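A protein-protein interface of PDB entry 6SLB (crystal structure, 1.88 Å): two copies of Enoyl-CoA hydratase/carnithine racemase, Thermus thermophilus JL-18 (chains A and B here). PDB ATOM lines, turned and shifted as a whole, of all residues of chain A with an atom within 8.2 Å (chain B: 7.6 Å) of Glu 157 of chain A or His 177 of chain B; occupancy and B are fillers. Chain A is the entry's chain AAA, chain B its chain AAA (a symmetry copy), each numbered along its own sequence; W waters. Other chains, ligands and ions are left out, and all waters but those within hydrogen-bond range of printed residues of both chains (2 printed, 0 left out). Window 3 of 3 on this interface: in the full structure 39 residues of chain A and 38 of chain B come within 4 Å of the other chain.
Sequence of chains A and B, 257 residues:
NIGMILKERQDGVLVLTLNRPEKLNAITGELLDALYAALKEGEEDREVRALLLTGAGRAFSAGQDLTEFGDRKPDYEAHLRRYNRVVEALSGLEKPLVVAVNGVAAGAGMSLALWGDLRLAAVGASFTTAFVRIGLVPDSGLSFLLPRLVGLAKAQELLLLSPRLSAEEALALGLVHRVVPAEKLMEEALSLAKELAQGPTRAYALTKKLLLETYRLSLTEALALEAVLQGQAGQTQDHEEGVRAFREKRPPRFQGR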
ATOM      1  N   THR A 129     -35.065   9.917   9.305  1.00  0.00           N
ATOM      2  CA  THR A 129     -36.182  10.541   8.559  1.00  0.00           C
ATOM      3  C   THR A 129     -37.081   9.433   7.991  1.00  0.00           C
ATOM      4  O   THR A 129     -38.283   9.622   8.047  1.00  0.00           O
ATOM      5  CB  THR A 129     -35.670  11.554   7.535  1.00  0.00           C
ATOM      6  OG1 THR A 129     -34.839  10.887   6.593  1.00  0.00           O
ATOM      7  CG2 THR A 129     -34.918  12.695   8.191  1.00  0.00           C
ATOM      8  N   VAL A 132     -37.999   8.503   2.767  1.00  0.00           N
ATOM      9  CA  VAL A 132     -37.414   8.273   1.420  1.00  0.00           C
ATOM     10  C   VAL A 132     -37.193   6.772   1.208  1.00  0.00           C
ATOM     11  O   VAL A 132     -37.328   6.322   0.054  1.00  0.00           O
ATOM     12  CB  VAL A 132     -36.140   9.110   1.186  1.00  0.00           C
ATOM     13  CG1 VAL A 132     -34.952   8.588   1.971  1.00  0.00           C
ATOM     14  CG2 VAL A 132     -35.833   9.174  -0.293  1.00  0.00           C
ATOM     15  N   LEU A 146     -37.520  20.609   9.907  1.00  0.00           N
ATOM     16  CA  LEU A 146     -36.124  20.122   9.838  1.00  0.00           C
ATOM     17  C   LEU A 146     -35.149  21.198   9.331  1.00  0.00           C
ATOM     18  O   LEU A 146     -34.131  21.445   9.989  1.00  0.00           O
ATOM     19  CB  LEU A 146     -36.037  18.811   9.050  1.00  0.00           C
ATOM     20  CG  LEU A 146     -34.692  18.093   9.205  1.00  0.00           C
ATOM     21  CD1 LEU A 146     -34.383  17.751  10.664  1.00  0.00           C
ATOM     22  CD2 LEU A 146     -34.647  16.826   8.353  1.00  0.00           C
ATOM     23  N   VAL A 150     -32.087  22.456  11.761  1.00  0.00           N
ATOM     24  CA  VAL A 150     -30.689  21.980  11.525  1.00  0.00           C
ATOM     25  C   VAL A 150     -30.048  22.709  10.332  1.00  0.00           C
ATOM     26  O   VAL A 150     -28.893  22.435  10.081  1.00  0.00           O
ATOM     27  CB  VAL A 150     -30.599  20.452  11.379  1.00  0.00           C
ATOM     28  CG1 VAL A 150     -31.156  19.770  12.620  1.00  0.00           C
ATOM     29  CG2 VAL A 150     -31.286  19.922  10.124  1.00  0.00           C
ATOM     30  N   GLY A 151     -30.743  23.648   9.710  1.00  0.00           N
ATOM     31  CA  GLY A 151     -30.270  24.345   8.501  1.00  0.00           C
ATOM     32  C   GLY A 151     -30.536  23.492   7.269  1.00  0.00           C
ATOM     33  O   GLY A 151     -30.668  22.274   7.380  1.00  0.00           O
ATOM     34  N   LEU A 152     -30.528  24.090   6.099  1.00  0.00           N
ATOM     35  CA  LEU A 152     -30.870  23.363   4.852  1.00  0.00           C
ATOM     36  C   LEU A 152     -29.815  22.305   4.517  1.00  0.00           C
ATOM     37  O   LEU A 152     -30.176  21.266   4.005  1.00  0.00           O
ATOM     38  CB  LEU A 152     -31.021  24.365   3.701  1.00  0.00           C
ATOM     39  CG  LEU A 152     -31.218  23.720   2.333  1.00  0.00           C
ATOM     40  CD1 LEU A 152     -32.507  22.909   2.354  1.00  0.00           C
ATOM     41  CD2 LEU A 152     -31.253  24.783   1.238  1.00  0.00           C
ATOM     42  N   ALA A 153     -28.524  22.535   4.738  1.00  0.00           N
ATOM     43  CA  ALA A 153     -27.478  21.572   4.334  1.00  0.00           C
ATOM     44  C   ALA A 153     -27.690  20.236   5.053  1.00  0.00           C
ATOM     45  O   ALA A 153     -27.647  19.130   4.416  1.00  0.00           O
ATOM     46  CB  ALA A 153     -26.093  22.138   4.590  1.00  0.00           C
ATOM     47  N   LYS A 154     -27.878  20.276   6.363  1.00  0.00           N
ATOM     48  CA  LYS A 154     -28.100  19.011   7.106  1.00  0.00           C
ATOM     49  C   LYS A 154     -29.474  18.405   6.745  1.00  0.00           C
ATOM     50  O   LYS A 154     -29.541  17.175   6.658  1.00  0.00           O
ATOM     51  CB  LYS A 154     -27.914  19.242   8.608  1.00  0.00           C
ATOM     52  CG  LYS A 154     -26.463  19.379   9.037  1.00  0.00           C
ATOM     53  CD  LYS A 154     -25.743  18.088   8.850  1.00  0.00           C
ATOM     54  CE  LYS A 154     -24.321  18.078   9.360  1.00  0.00           C
ATOM     55  NZ  LYS A 154     -23.693  16.786   9.016  1.00  0.00           N
ATOM     56  N   ALA A 155     -30.529  19.214   6.556  1.00  0.00           N
ATOM     57  CA  ALA A 155     -31.884  18.722   6.208  1.00  0.00           C
ATOM     58  C   ALA A 155     -31.816  17.933   4.893  1.00  0.00           C
ATOM     59  O   ALA A 155     -32.333  16.805   4.832  1.00  0.00           O
ATOM     60  CB  ALA A 155     -32.850  19.860   6.121  1.00  0.00           C
ATOM     61  N   GLN A 156     -31.059  18.426   3.911  1.00  0.00           N
ATOM     62  CA  GLN A 156     -30.915  17.735   2.588  1.00  0.00           C
ATOM     63  C   GLN A 156     -30.334  16.333   2.780  1.00  0.00           C
ATOM     64  O   GLN A 156     -30.857  15.342   2.195  1.00  0.00           O
ATOM     65  CB  GLN A 156     -29.934  18.464   1.660  1.00  0.00           C
ATOM     66  CG  GLN A 156     -30.428  19.804   1.197  1.00  0.00           C
ATOM     67  CD  GLN A 156     -29.340  20.580   0.494  1.00  0.00           C
ATOM     68  OE1 GLN A 156     -28.202  20.685   0.949  1.00  0.00           O
ATOM     69  NE2 GLN A 156     -29.722  21.175  -0.615  1.00  0.00           N
ATOM     70  N   GLU A 157     -29.234  16.250   3.516  1.00  0.00           N
ATOM     71  CA  GLU A 157     -28.527  14.977   3.768  1.00  0.00           C
ATOM     72  C   GLU A 157     -29.433  14.034   4.572  1.00  0.00           C
ATOM     73  O   GLU A 157     -29.563  12.830   4.229  1.00  0.00           O
ATOM     74  CB  GLU A 157     -27.236  15.296   4.509  1.00  0.00           C
ATOM     75  CG  GLU A 157     -26.305  14.120   4.651  1.00  0.00           C
ATOM     76  CD  GLU A 157     -24.978  14.509   5.305  1.00  0.00           C
ATOM     77  OE1 GLU A 157     -24.932  15.552   6.011  1.00  0.00           O
ATOM     78  OE2 GLU A 157     -23.995  13.782   5.093  1.00  0.00           O
ATOM     79  N   LEU A 158     -30.030  14.541   5.642  1.00  0.00           N
ATOM     80  CA  LEU A 158     -30.865  13.686   6.527  1.00  0.00           C
ATOM     81  C   LEU A 158     -32.076  13.124   5.748  1.00  0.00           C
ATOM     82  O   LEU A 158     -32.440  11.960   5.981  1.00  0.00           O
ATOM     83  CB  LEU A 158     -31.305  14.483   7.745  1.00  0.00           C
ATOM     84  CG  LEU A 158     -30.210  14.833   8.751  1.00  0.00           C
ATOM     85  CD1 LEU A 158     -30.824  15.478   9.978  1.00  0.00           C
ATOM     86  CD2 LEU A 158     -29.394  13.630   9.124  1.00  0.00           C
ATOM     87  N   LEU A 159     -32.678  13.911   4.871  1.00  0.00           N
ATOM     88  CA  LEU A 159     -33.930  13.550   4.196  1.00  0.00           C
ATOM     89  C   LEU A 159     -33.622  12.663   2.990  1.00  0.00           C
ATOM     90  O   LEU A 159     -34.351  11.648   2.817  1.00  0.00           O
ATOM     91  CB  LEU A 159     -34.659  14.828   3.801  1.00  0.00           C
ATOM     92  CG  LEU A 159     -35.336  15.568   4.948  1.00  0.00           C
ATOM     93  CD1 LEU A 159     -35.856  16.893   4.470  1.00  0.00           C
ATOM     94  CD2 LEU A 159     -36.481  14.710   5.504  1.00  0.00           C
ATOM     95  N   LEU A 160     -32.621  13.026   2.175  1.00  0.00           N
ATOM     96  CA  LEU A 160     -32.301  12.309   0.915  1.00  0.00           C
ATOM     97  C   LEU A 160     -31.640  10.953   1.180  1.00  0.00           C
ATOM     98  O   LEU A 160     -31.947   9.983   0.420  1.00  0.00           O
ATOM     99  CB  LEU A 160     -31.435  13.205   0.013  1.00  0.00           C
ATOM    100  CG  LEU A 160     -32.130  14.492  -0.427  1.00  0.00           C
ATOM    101  CD1 LEU A 160     -31.210  15.357  -1.275  1.00  0.00           C
ATOM    102  CD2 LEU A 160     -33.458  14.210  -1.152  1.00  0.00           C
ATOM    103  N   LEU A 161     -30.792  10.843   2.210  1.00  0.00           N
ATOM    104  CA  LEU A 161     -29.991   9.638   2.493  1.00  0.00           C
ATOM    105  C   LEU A 161     -30.586   8.864   3.683  1.00  0.00           C
ATOM    106  O   LEU A 161     -30.173   7.757   3.898  1.00  0.00           O
ATOM    107  CB  LEU A 161     -28.542  10.081   2.736  1.00  0.00           C
ATOM    108  CG  LEU A 161     -27.858  10.694   1.513  1.00  0.00           C
ATOM    109  CD1 LEU A 161     -26.412  11.071   1.822  1.00  0.00           C
ATOM    110  CD2 LEU A 161     -27.915   9.724   0.325  1.00  0.00           C
ATOM    111  N   SER A 162     -31.475   9.457   4.470  1.00  0.00           N
ATOM    112  CA  SER A 162     -32.098   8.809   5.657  1.00  0.00           C
ATOM    113  C   SER A 162     -31.080   8.026   6.487  1.00  0.00           C
ATOM    114  O   SER A 162     -31.349   6.876   6.835  1.00  0.00           O
ATOM    115  CB  SER A 162     -33.246   7.909   5.244  1.00  0.00           C
ATOM    116  OG  SER A 162     -33.923   7.402   6.385  1.00  0.00           O
ATOM    117  N   PRO A 163     -29.957   8.641   6.928  1.00  0.00           N
ATOM    118  CA  PRO A 163     -29.060   8.011   7.884  1.00  0.00           C
ATOM    119  C   PRO A 163     -29.757   7.912   9.249  1.00  0.00           C
ATOM    120  O   PRO A 163     -30.751   8.615   9.507  1.00  0.00           O
ATOM    121  CB  PRO A 163     -27.861   8.964   7.943  1.00  0.00           C
ATOM    122  CG  PRO A 163     -28.473  10.304   7.659  1.00  0.00           C
ATOM    123  CD  PRO A 163     -29.505  10.005   6.605  1.00  0.00           C
ATOM    124  N   LEU A 165     -29.252   8.661  13.058  1.00  0.00           N
ATOM    125  CA  LEU A 165     -28.457   9.578  13.909  1.00  0.00           C
ATOM    126  C   LEU A 165     -28.502   9.081  15.344  1.00  0.00           C
ATOM    127  O   LEU A 165     -29.611   8.841  15.845  1.00  0.00           O
ATOM    128  CB  LEU A 165     -29.045  10.983  13.811  1.00  0.00           C
ATOM    129  CG  LEU A 165     -29.232  11.452  12.374  1.00  0.00           C
ATOM    130  CD1 LEU A 165     -30.032  12.735  12.337  1.00  0.00           C
ATOM    131  CD2 LEU A 165     -27.875  11.620  11.705  1.00  0.00           C
ATOM    132  N   LEU A 173     -26.611  18.524  16.118  1.00  0.00           N
ATOM    133  CA  LEU A 173     -27.327  19.185  14.982  1.00  0.00           C
ATOM    134  C   LEU A 173     -28.396  20.142  15.502  1.00  0.00           C
ATOM    135  O   LEU A 173     -28.878  20.930  14.691  1.00  0.00           O
ATOM    136  CB  LEU A 173     -27.976  18.121  14.106  1.00  0.00           C
ATOM    137  CG  LEU A 173     -27.023  17.108  13.489  1.00  0.00           C
ATOM    138  CD1 LEU A 173     -27.775  16.101  12.659  1.00  0.00           C
ATOM    139  CD2 LEU A 173     -25.971  17.796  12.636  1.00  0.00           C
ATOM    140  N   VAL B  99     -22.771  17.423  -6.598  1.00  0.00           N
ATOM    141  CA  VAL B  99     -21.681  18.331  -7.032  1.00  0.00           C
ATOM    142  C   VAL B  99     -20.350  17.837  -6.449  1.00  0.00           C
ATOM    143  O   VAL B  99     -20.283  17.566  -5.244  1.00  0.00           O
ATOM    144  CB  VAL B  99     -21.996  19.800  -6.713  1.00  0.00           C
ATOM    145  CG1 VAL B  99     -20.798  20.719  -6.918  1.00  0.00           C
ATOM    146  CG2 VAL B  99     -23.168  20.293  -7.558  1.00  0.00           C
ATOM    147  N   LEU B 114     -23.402  25.191  -5.000  1.00  0.00           N
ATOM    148  CA  LEU B 114     -24.261  25.077  -3.782  1.00  0.00           C
ATOM    149  C   LEU B 114     -25.660  24.594  -4.178  1.00  0.00           C
ATOM    150  O   LEU B 114     -26.431  24.183  -3.276  1.00  0.00           O
ATOM    151  CB  LEU B 114     -24.299  26.435  -3.076  1.00  0.00           C
ATOM    152  CG  LEU B 114     -22.995  26.850  -2.402  1.00  0.00           C
ATOM    153  CD1 LEU B 114     -23.204  28.065  -1.498  1.00  0.00           C
ATOM    154  CD2 LEU B 114     -22.388  25.706  -1.607  1.00  0.00           C
ATOM    155  N   GLY B 116     -26.091  21.814  -5.763  1.00  0.00           N
ATOM    156  CA  GLY B 116     -26.048  20.361  -5.534  1.00  0.00           C
ATOM    157  C   GLY B 116     -26.952  19.960  -4.388  1.00  0.00           C
ATOM    158  O   GLY B 116     -26.919  20.662  -3.386  1.00  0.00           O
ATOM    159  N   ASP B 117     -27.670  18.836  -4.489  1.00  0.00           N
ATOM    160  CA  ASP B 117     -28.403  18.228  -3.339  1.00  0.00           C
ATOM    161  C   ASP B 117     -27.431  17.640  -2.334  1.00  0.00           C
ATOM    162  O   ASP B 117     -27.626  17.853  -1.095  1.00  0.00           O
ATOM    163  CB  ASP B 117     -29.354  17.147  -3.841  1.00  0.00           C
ATOM    164  CG  ASP B 117     -30.388  17.747  -4.773  1.00  0.00           C
ATOM    165  OD1 ASP B 117     -31.011  18.785  -4.352  1.00  0.00           O
ATOM    166  OD2 ASP B 117     -30.556  17.189  -5.906  1.00  0.00           O
ATOM    167  N   LEU B 118     -26.417  16.943  -2.838  1.00  0.00           N
ATOM    168  CA  LEU B 118     -25.290  16.418  -2.028  1.00  0.00           C
ATOM    169  C   LEU B 118     -23.997  16.963  -2.642  1.00  0.00           C
ATOM    170  O   LEU B 118     -23.852  16.943  -3.872  1.00  0.00           O
ATOM    171  CB  LEU B 118     -25.297  14.893  -2.010  1.00  0.00           C
ATOM    172  CG  LEU B 118     -26.287  14.195  -1.067  1.00  0.00           C
ATOM    173  CD1 LEU B 118     -26.226  14.767   0.328  1.00  0.00           C
ATOM    174  CD2 LEU B 118     -27.687  14.223  -1.628  1.00  0.00           C
ATOM    175  N   ARG B 119     -23.113  17.488  -1.802  1.00  0.00           N
ATOM    176  CA  ARG B 119     -21.939  18.236  -2.253  1.00  0.00           C
ATOM    177  C   ARG B 119     -20.702  17.619  -1.596  1.00  0.00           C
ATOM    178  O   ARG B 119     -20.700  17.484  -0.358  1.00  0.00           O
ATOM    179  CB  ARG B 119     -22.126  19.718  -1.906  1.00  0.00           C
ATOM    180  CG  ARG B 119     -23.330  20.362  -2.584  1.00  0.00           C
ATOM    181  CD  ARG B 119     -23.615  21.808  -2.246  1.00  0.00           C
ATOM    182  NE  ARG B 119     -23.804  21.958  -0.803  1.00  0.00           N
ATOM    183  CZ  ARG B 119     -24.922  21.680  -0.151  1.00  0.00           C
ATOM    184  NH1 ARG B 119     -26.003  21.293  -0.807  1.00  0.00           N
ATOM    185  NH2 ARG B 119     -24.969  21.816   1.165  1.00  0.00           N
ATOM    186  N   LEU B 120     -19.718  17.264  -2.405  1.00  0.00           N
ATOM    187  CA  LEU B 120     -18.410  16.742  -1.952  1.00  0.00           C
ATOM    188  C   LEU B 120     -17.355  17.742  -2.418  1.00  0.00           C
ATOM    189  O   LEU B 120     -17.521  18.337  -3.517  1.00  0.00           O
ATOM    190  CB  LEU B 120     -18.109  15.379  -2.566  1.00  0.00           C
ATOM    191  CG  LEU B 120     -18.943  14.204  -2.071  1.00  0.00           C
ATOM    192  CD1 LEU B 120     -20.370  14.308  -2.564  1.00  0.00           C
ATOM    193  CD2 LEU B 120     -18.297  12.908  -2.523  1.00  0.00           C
ATOM    194  N   ALA B 121     -16.286  17.906  -1.650  1.00  0.00           N
ATOM    195  CA  ALA B 121     -15.149  18.752  -2.081  1.00  0.00           C
ATOM    196  C   ALA B 121     -13.857  17.939  -2.004  1.00  0.00           C
ATOM    197  O   ALA B 121     -13.705  17.120  -1.073  1.00  0.00           O
ATOM    198  CB  ALA B 121     -15.029  19.987  -1.232  1.00  0.00           C
ATOM    199  N   LEU B 149     -28.338  27.552   3.911  1.00  0.00           N
ATOM    200  CA  LEU B 149     -27.283  26.519   4.084  1.00  0.00           C
ATOM    201  C   LEU B 149     -26.445  26.737   5.342  1.00  0.00           C
ATOM    202  O   LEU B 149     -26.126  25.711   5.984  1.00  0.00           O
ATOM    203  CB  LEU B 149     -26.378  26.455   2.857  1.00  0.00           C
ATOM    204  CG  LEU B 149     -27.045  25.948   1.581  1.00  0.00           C
ATOM    205  CD1 LEU B 149     -26.074  26.069   0.400  1.00  0.00           C
ATOM    206  CD2 LEU B 149     -27.519  24.511   1.743  1.00  0.00           C
ATOM    207  N   ALA B 170     -15.416  24.655   4.851  1.00  0.00           N
ATOM    208  CA  ALA B 170     -16.682  24.525   4.101  1.00  0.00           C
ATOM    209  C   ALA B 170     -17.482  23.388   4.714  1.00  0.00           C
ATOM    210  O   ALA B 170     -18.689  23.540   4.882  1.00  0.00           O
ATOM    211  CB  ALA B 170     -16.393  24.271   2.636  1.00  0.00           C
ATOM    212  N   LEU B 171     -16.806  22.277   5.013  1.00  0.00           N
ATOM    213  CA  LEU B 171     -17.426  21.098   5.661  1.00  0.00           C
ATOM    214  C   LEU B 171     -18.055  21.549   6.984  1.00  0.00           C
ATOM    215  O   LEU B 171     -19.239  21.242   7.218  1.00  0.00           O
ATOM    216  CB  LEU B 171     -16.374  20.007   5.860  1.00  0.00           C
ATOM    217  CG  LEU B 171     -16.902  18.686   6.419  1.00  0.00           C
ATOM    218  CD1 LEU B 171     -17.939  18.051   5.492  1.00  0.00           C
ATOM    219  CD2 LEU B 171     -15.746  17.719   6.705  1.00  0.00           C
ATOM    220  N   GLY B 174     -21.363  23.573   6.426  1.00  0.00           N
ATOM    221  CA  GLY B 174     -22.441  22.941   5.641  1.00  0.00           C
ATOM    222  C   GLY B 174     -22.404  23.317   4.169  1.00  0.00           C
ATOM    223  O   GLY B 174     -23.306  22.903   3.414  1.00  0.00           O
ATOM    224  N   LEU B 175     -21.361  23.985   3.707  1.00  0.00           N
ATOM    225  CA  LEU B 175     -21.230  24.270   2.257  1.00  0.00           C
ATOM    226  C   LEU B 175     -21.044  22.947   1.513  1.00  0.00           C
ATOM    227  O   LEU B 175     -21.454  22.831   0.366  1.00  0.00           O
ATOM    228  CB  LEU B 175     -20.026  25.176   2.044  1.00  0.00           C
ATOM    229  CG  LEU B 175     -20.189  26.601   2.559  1.00  0.00           C
ATOM    230  CD1 LEU B 175     -18.968  27.402   2.197  1.00  0.00           C
ATOM    231  CD2 LEU B 175     -21.448  27.237   1.993  1.00  0.00           C
ATOM    232  N   VAL B 176     -20.369  21.991   2.129  1.00  0.00           N
ATOM    233  CA  VAL B 176     -20.272  20.632   1.546  1.00  0.00           C
ATOM    234  C   VAL B 176     -20.634  19.647   2.636  1.00  0.00           C
ATOM    235  O   VAL B 176     -20.612  20.047   3.824  1.00  0.00           O
ATOM    236  CB  VAL B 176     -18.901  20.314   0.935  1.00  0.00           C
ATOM    237  CG1 VAL B 176     -18.578  21.280  -0.177  1.00  0.00           C
ATOM    238  CG2 VAL B 176     -17.784  20.197   1.979  1.00  0.00           C
ATOM    239  N   HIS B 177     -20.911  18.415   2.206  1.00  0.00           N
ATOM    240  CA  HIS B 177     -21.308  17.280   3.067  1.00  0.00           C
ATOM    241  C   HIS B 177     -20.120  16.363   3.348  1.00  0.00           C
ATOM    242  O   HIS B 177     -20.170  15.645   4.348  1.00  0.00           O
ATOM    243  CB  HIS B 177     -22.467  16.512   2.442  1.00  0.00           C
ATOM    244  CG  HIS B 177     -23.704  17.310   2.260  1.00  0.00           C
ATOM    245  ND1 HIS B 177     -24.082  17.778   1.026  1.00  0.00           N
ATOM    246  CD2 HIS B 177     -24.677  17.692   3.124  1.00  0.00           C
ATOM    247  CE1 HIS B 177     -25.248  18.395   1.145  1.00  0.00           C
ATOM    248  NE2 HIS B 177     -25.622  18.364   2.399  1.00  0.00           N
ATOM    249  N   ARG B 178     -19.103  16.365   2.508  1.00  0.00           N
ATOM    250  CA  ARG B 178     -17.976  15.417   2.619  1.00  0.00           C
ATOM    251  C   ARG B 178     -16.740  16.061   1.999  1.00  0.00           C
ATOM    252  O   ARG B 178     -16.899  16.800   1.033  1.00  0.00           O
ATOM    253  CB  ARG B 178     -18.336  14.078   1.974  1.00  0.00           C
ATOM    254  CG  ARG B 178     -17.232  13.033   2.071  1.00  0.00           C
ATOM    255  CD  ARG B 178     -17.730  11.616   2.348  1.00  0.00           C
ATOM    256  NE  ARG B 178     -18.859  11.230   1.501  1.00  0.00           N
ATOM    257  CZ  ARG B 178     -18.825  10.331   0.503  1.00  0.00           C
ATOM    258  NH1 ARG B 178     -17.703   9.688   0.202  1.00  0.00           N
ATOM    259  NH2 ARG B 178     -19.933  10.057  -0.177  1.00  0.00           N
ATOM    260  N   VAL B 179     -15.569  15.836   2.591  1.00  0.00           N
ATOM    261  CA  VAL B 179     -14.279  16.245   1.972  1.00  0.00           C
ATOM    262  C   VAL B 179     -13.473  14.972   1.719  1.00  0.00           C
ATOM    263  O   VAL B 179     -13.440  14.139   2.627  1.00  0.00           O
ATOM    264  CB  VAL B 179     -13.515  17.226   2.860  1.00  0.00           C
ATOM    265  CG1 VAL B 179     -12.084  17.376   2.392  1.00  0.00           C
ATOM    266  CG2 VAL B 179     -14.241  18.557   2.945  1.00  0.00           C
ATOM    267  N   LEU B 192     -21.547   7.877  -5.101  1.00  0.00           N
ATOM    268  CA  LEU B 192     -22.756   8.415  -4.430  1.00  0.00           C
ATOM    269  C   LEU B 192     -23.844   8.629  -5.491  1.00  0.00           C
ATOM    270  O   LEU B 192     -25.005   8.260  -5.202  1.00  0.00           O
ATOM    271  CB  LEU B 192     -22.421   9.719  -3.702  1.00  0.00           C
ATOM    272  CG  LEU B 192     -23.618  10.472  -3.116  1.00  0.00           C
ATOM    273  CD1 LEU B 192     -24.317   9.642  -2.065  1.00  0.00           C
ATOM    274  CD2 LEU B 192     -23.181  11.817  -2.559  1.00  0.00           C
ATOM    275  N   LEU B 211     -38.420  21.363   0.142  1.00  0.00           N
ATOM    276  CA  LEU B 211     -37.246  22.092   0.701  1.00  0.00           C
ATOM    277  C   LEU B 211     -37.131  23.479   0.080  1.00  0.00           C
ATOM    278  O   LEU B 211     -36.845  24.411   0.831  1.00  0.00           O
ATOM    279  CB  LEU B 211     -35.960  21.296   0.487  1.00  0.00           C
ATOM    280  CG  LEU B 211     -35.871  20.067   1.376  1.00  0.00           C
ATOM    281  CD1 LEU B 211     -34.614  19.284   1.138  1.00  0.00           C
ATOM    282  CD2 LEU B 211     -36.013  20.464   2.821  1.00  0.00           C
HETATM  283  O   HOH W   1     -28.580  22.998  -2.550  1.00  0.00           O
HETATM  284  O   HOH W   2     -32.135  19.840  -2.047  1.00  0.00           O
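The guanidinium group of Arg 119 of chain B sits at hydrogen-bond distance from the side-chain amide oxygen of Gln 156 of chain A, 2.9 Å away.
The backbone carbonyl oxygen (O) of Ala 153 of chain A sits at hydrogen-bond distance from a ring nitrogen (NE2) of His 177 of chain B, 3.0 Å away.
O of Arg 119 of chain B is in hydrogen-bond range of N of Arg 178 of chain B (3.5 Å).
The backbone carbonyl oxygen (O) of Arg 119 of chain B sits at hydrogen-bond distance from the backbone NH (N) of His 177 of chain B (2.7 Å).
O of Gly 116 of chain B lies within hydrogen-bond range of NH1 of Arg 119 of chain B (2.8 Å).
The side-chain carboxylate of Glu 157 of chain A lies within salt-bridge range of the side-chain amino group of Lys 154 of chain A (3.5 Å).
The backbone NH (N) of Val 99 of chain B lies within hydrogen-bond range of the backbone carbonyl oxygen (O) of Leu 118 of chain B.
The backbone carbonyl oxygen of Gly 174 of chain B lies within hydrogen-bond range of the guanidinium group of Arg 119 of chain B (3.0 Å).
Among the printed residues, pairs that only touch across the chains: Ala 153 of chain A with Gly 174 of chain B (3.1 Å), Gln 156 of chain A with Asp 117 of chain B (3.5 Å), Glu 157 of chain A with His 177 of chain B (3.6 Å), Ala 153 of chain A with Arg 119 of chain B (3.6 Å), Leu 160 of chain A with Asp 117 of chain B (3.6 Å), Leu 160 of chain A with Leu 118 of chain B (3.7 Å), Ala 153 of chain A with Leu 149 of chain B (3.7 Å), Gln 156 of chain A with His 177 of chain B (3.7 Å), Leu 152 of chain A with Leu 149 of chain B (3.8 Å), Leu 159 of chain A with Leu 211 of chain B (3.9 Å), Gln 156 of chain A with Leu 149 of chain B (3.97 Å), Gln 156 of chain A with Gly 116 of chain B (3.97 Å) and Leu 161 of chain A with Leu 118 of chain B (3.99 Å).
Of chain B, only His 177 (3.6 Å) comes within 4 Å of Glu 157 of chain A.
Printed residues of chain B within 4 Å of Leu 160 of chain A: Asp 117 and Leu 118.
Leu 165 of chain A touches none of the printed residues of chain B.
Printed residues of chain A within 4 Å of Leu 118 of chain B: Leu 160 and Leu 161.
Of the printed residues of chain A, Arg 119 of chain B touches Ala 153 (3.6 Å) and Gln 156 (2.9 Å).
Of the printed residues of chain A, Leu 149 of chain B touches Leu 152, Ala 153 and Gln 156.
Of the printed residues of chain A, Gly 174 of chain B touches Ala 153.
Of chain A, only Ala 153 (3.0 Å), Gln 156 (3.7 Å) and Glu 157 (3.6 Å) come within 4 Å of His 177 of chain B.
The nearest residue of chain A that does not touch His 177 of chain B is Lys 154 of chain A (4.9 Å).
The nearest printed residue of chain B that does not touch Gln 156 of chain A is Leu 211 of chain B (4.2 Å).
Of the 19 printed residues of chain B, 8 touch a printed residue of chain A.
Hydrophobic or aromatic side chains of chain B that line the printed part of chain A: Leu 118, Leu 149, His 177 and Leu 211.
Among the printed residues, 15 pairs touch across the chains.
Among the printed residues, no Asp or Glu carboxylate lies within 4 Å of a Lys or Arg side-chain nitrogen of the other chain.
No position is printed for both chains.
Of the 15 pairs that touch across the chains among the printed residues, none has its exchanged pair printed and touching as well.
Water W1 lies within hydrogen-bond range of the backbone carbonyl oxygen (O) of Leu 114 of chain B, the side-chain amide nitrogen (NE2) of Gln 156 of chain A and the backbone carbonyl oxygen (O) of Gly 116 of chain B.
Water W2 lies within hydrogen-bond range of OD1 of Asp 117 of chain B (2.8 Å) and NE2 of Gln 156 of chain A (3.1 Å).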
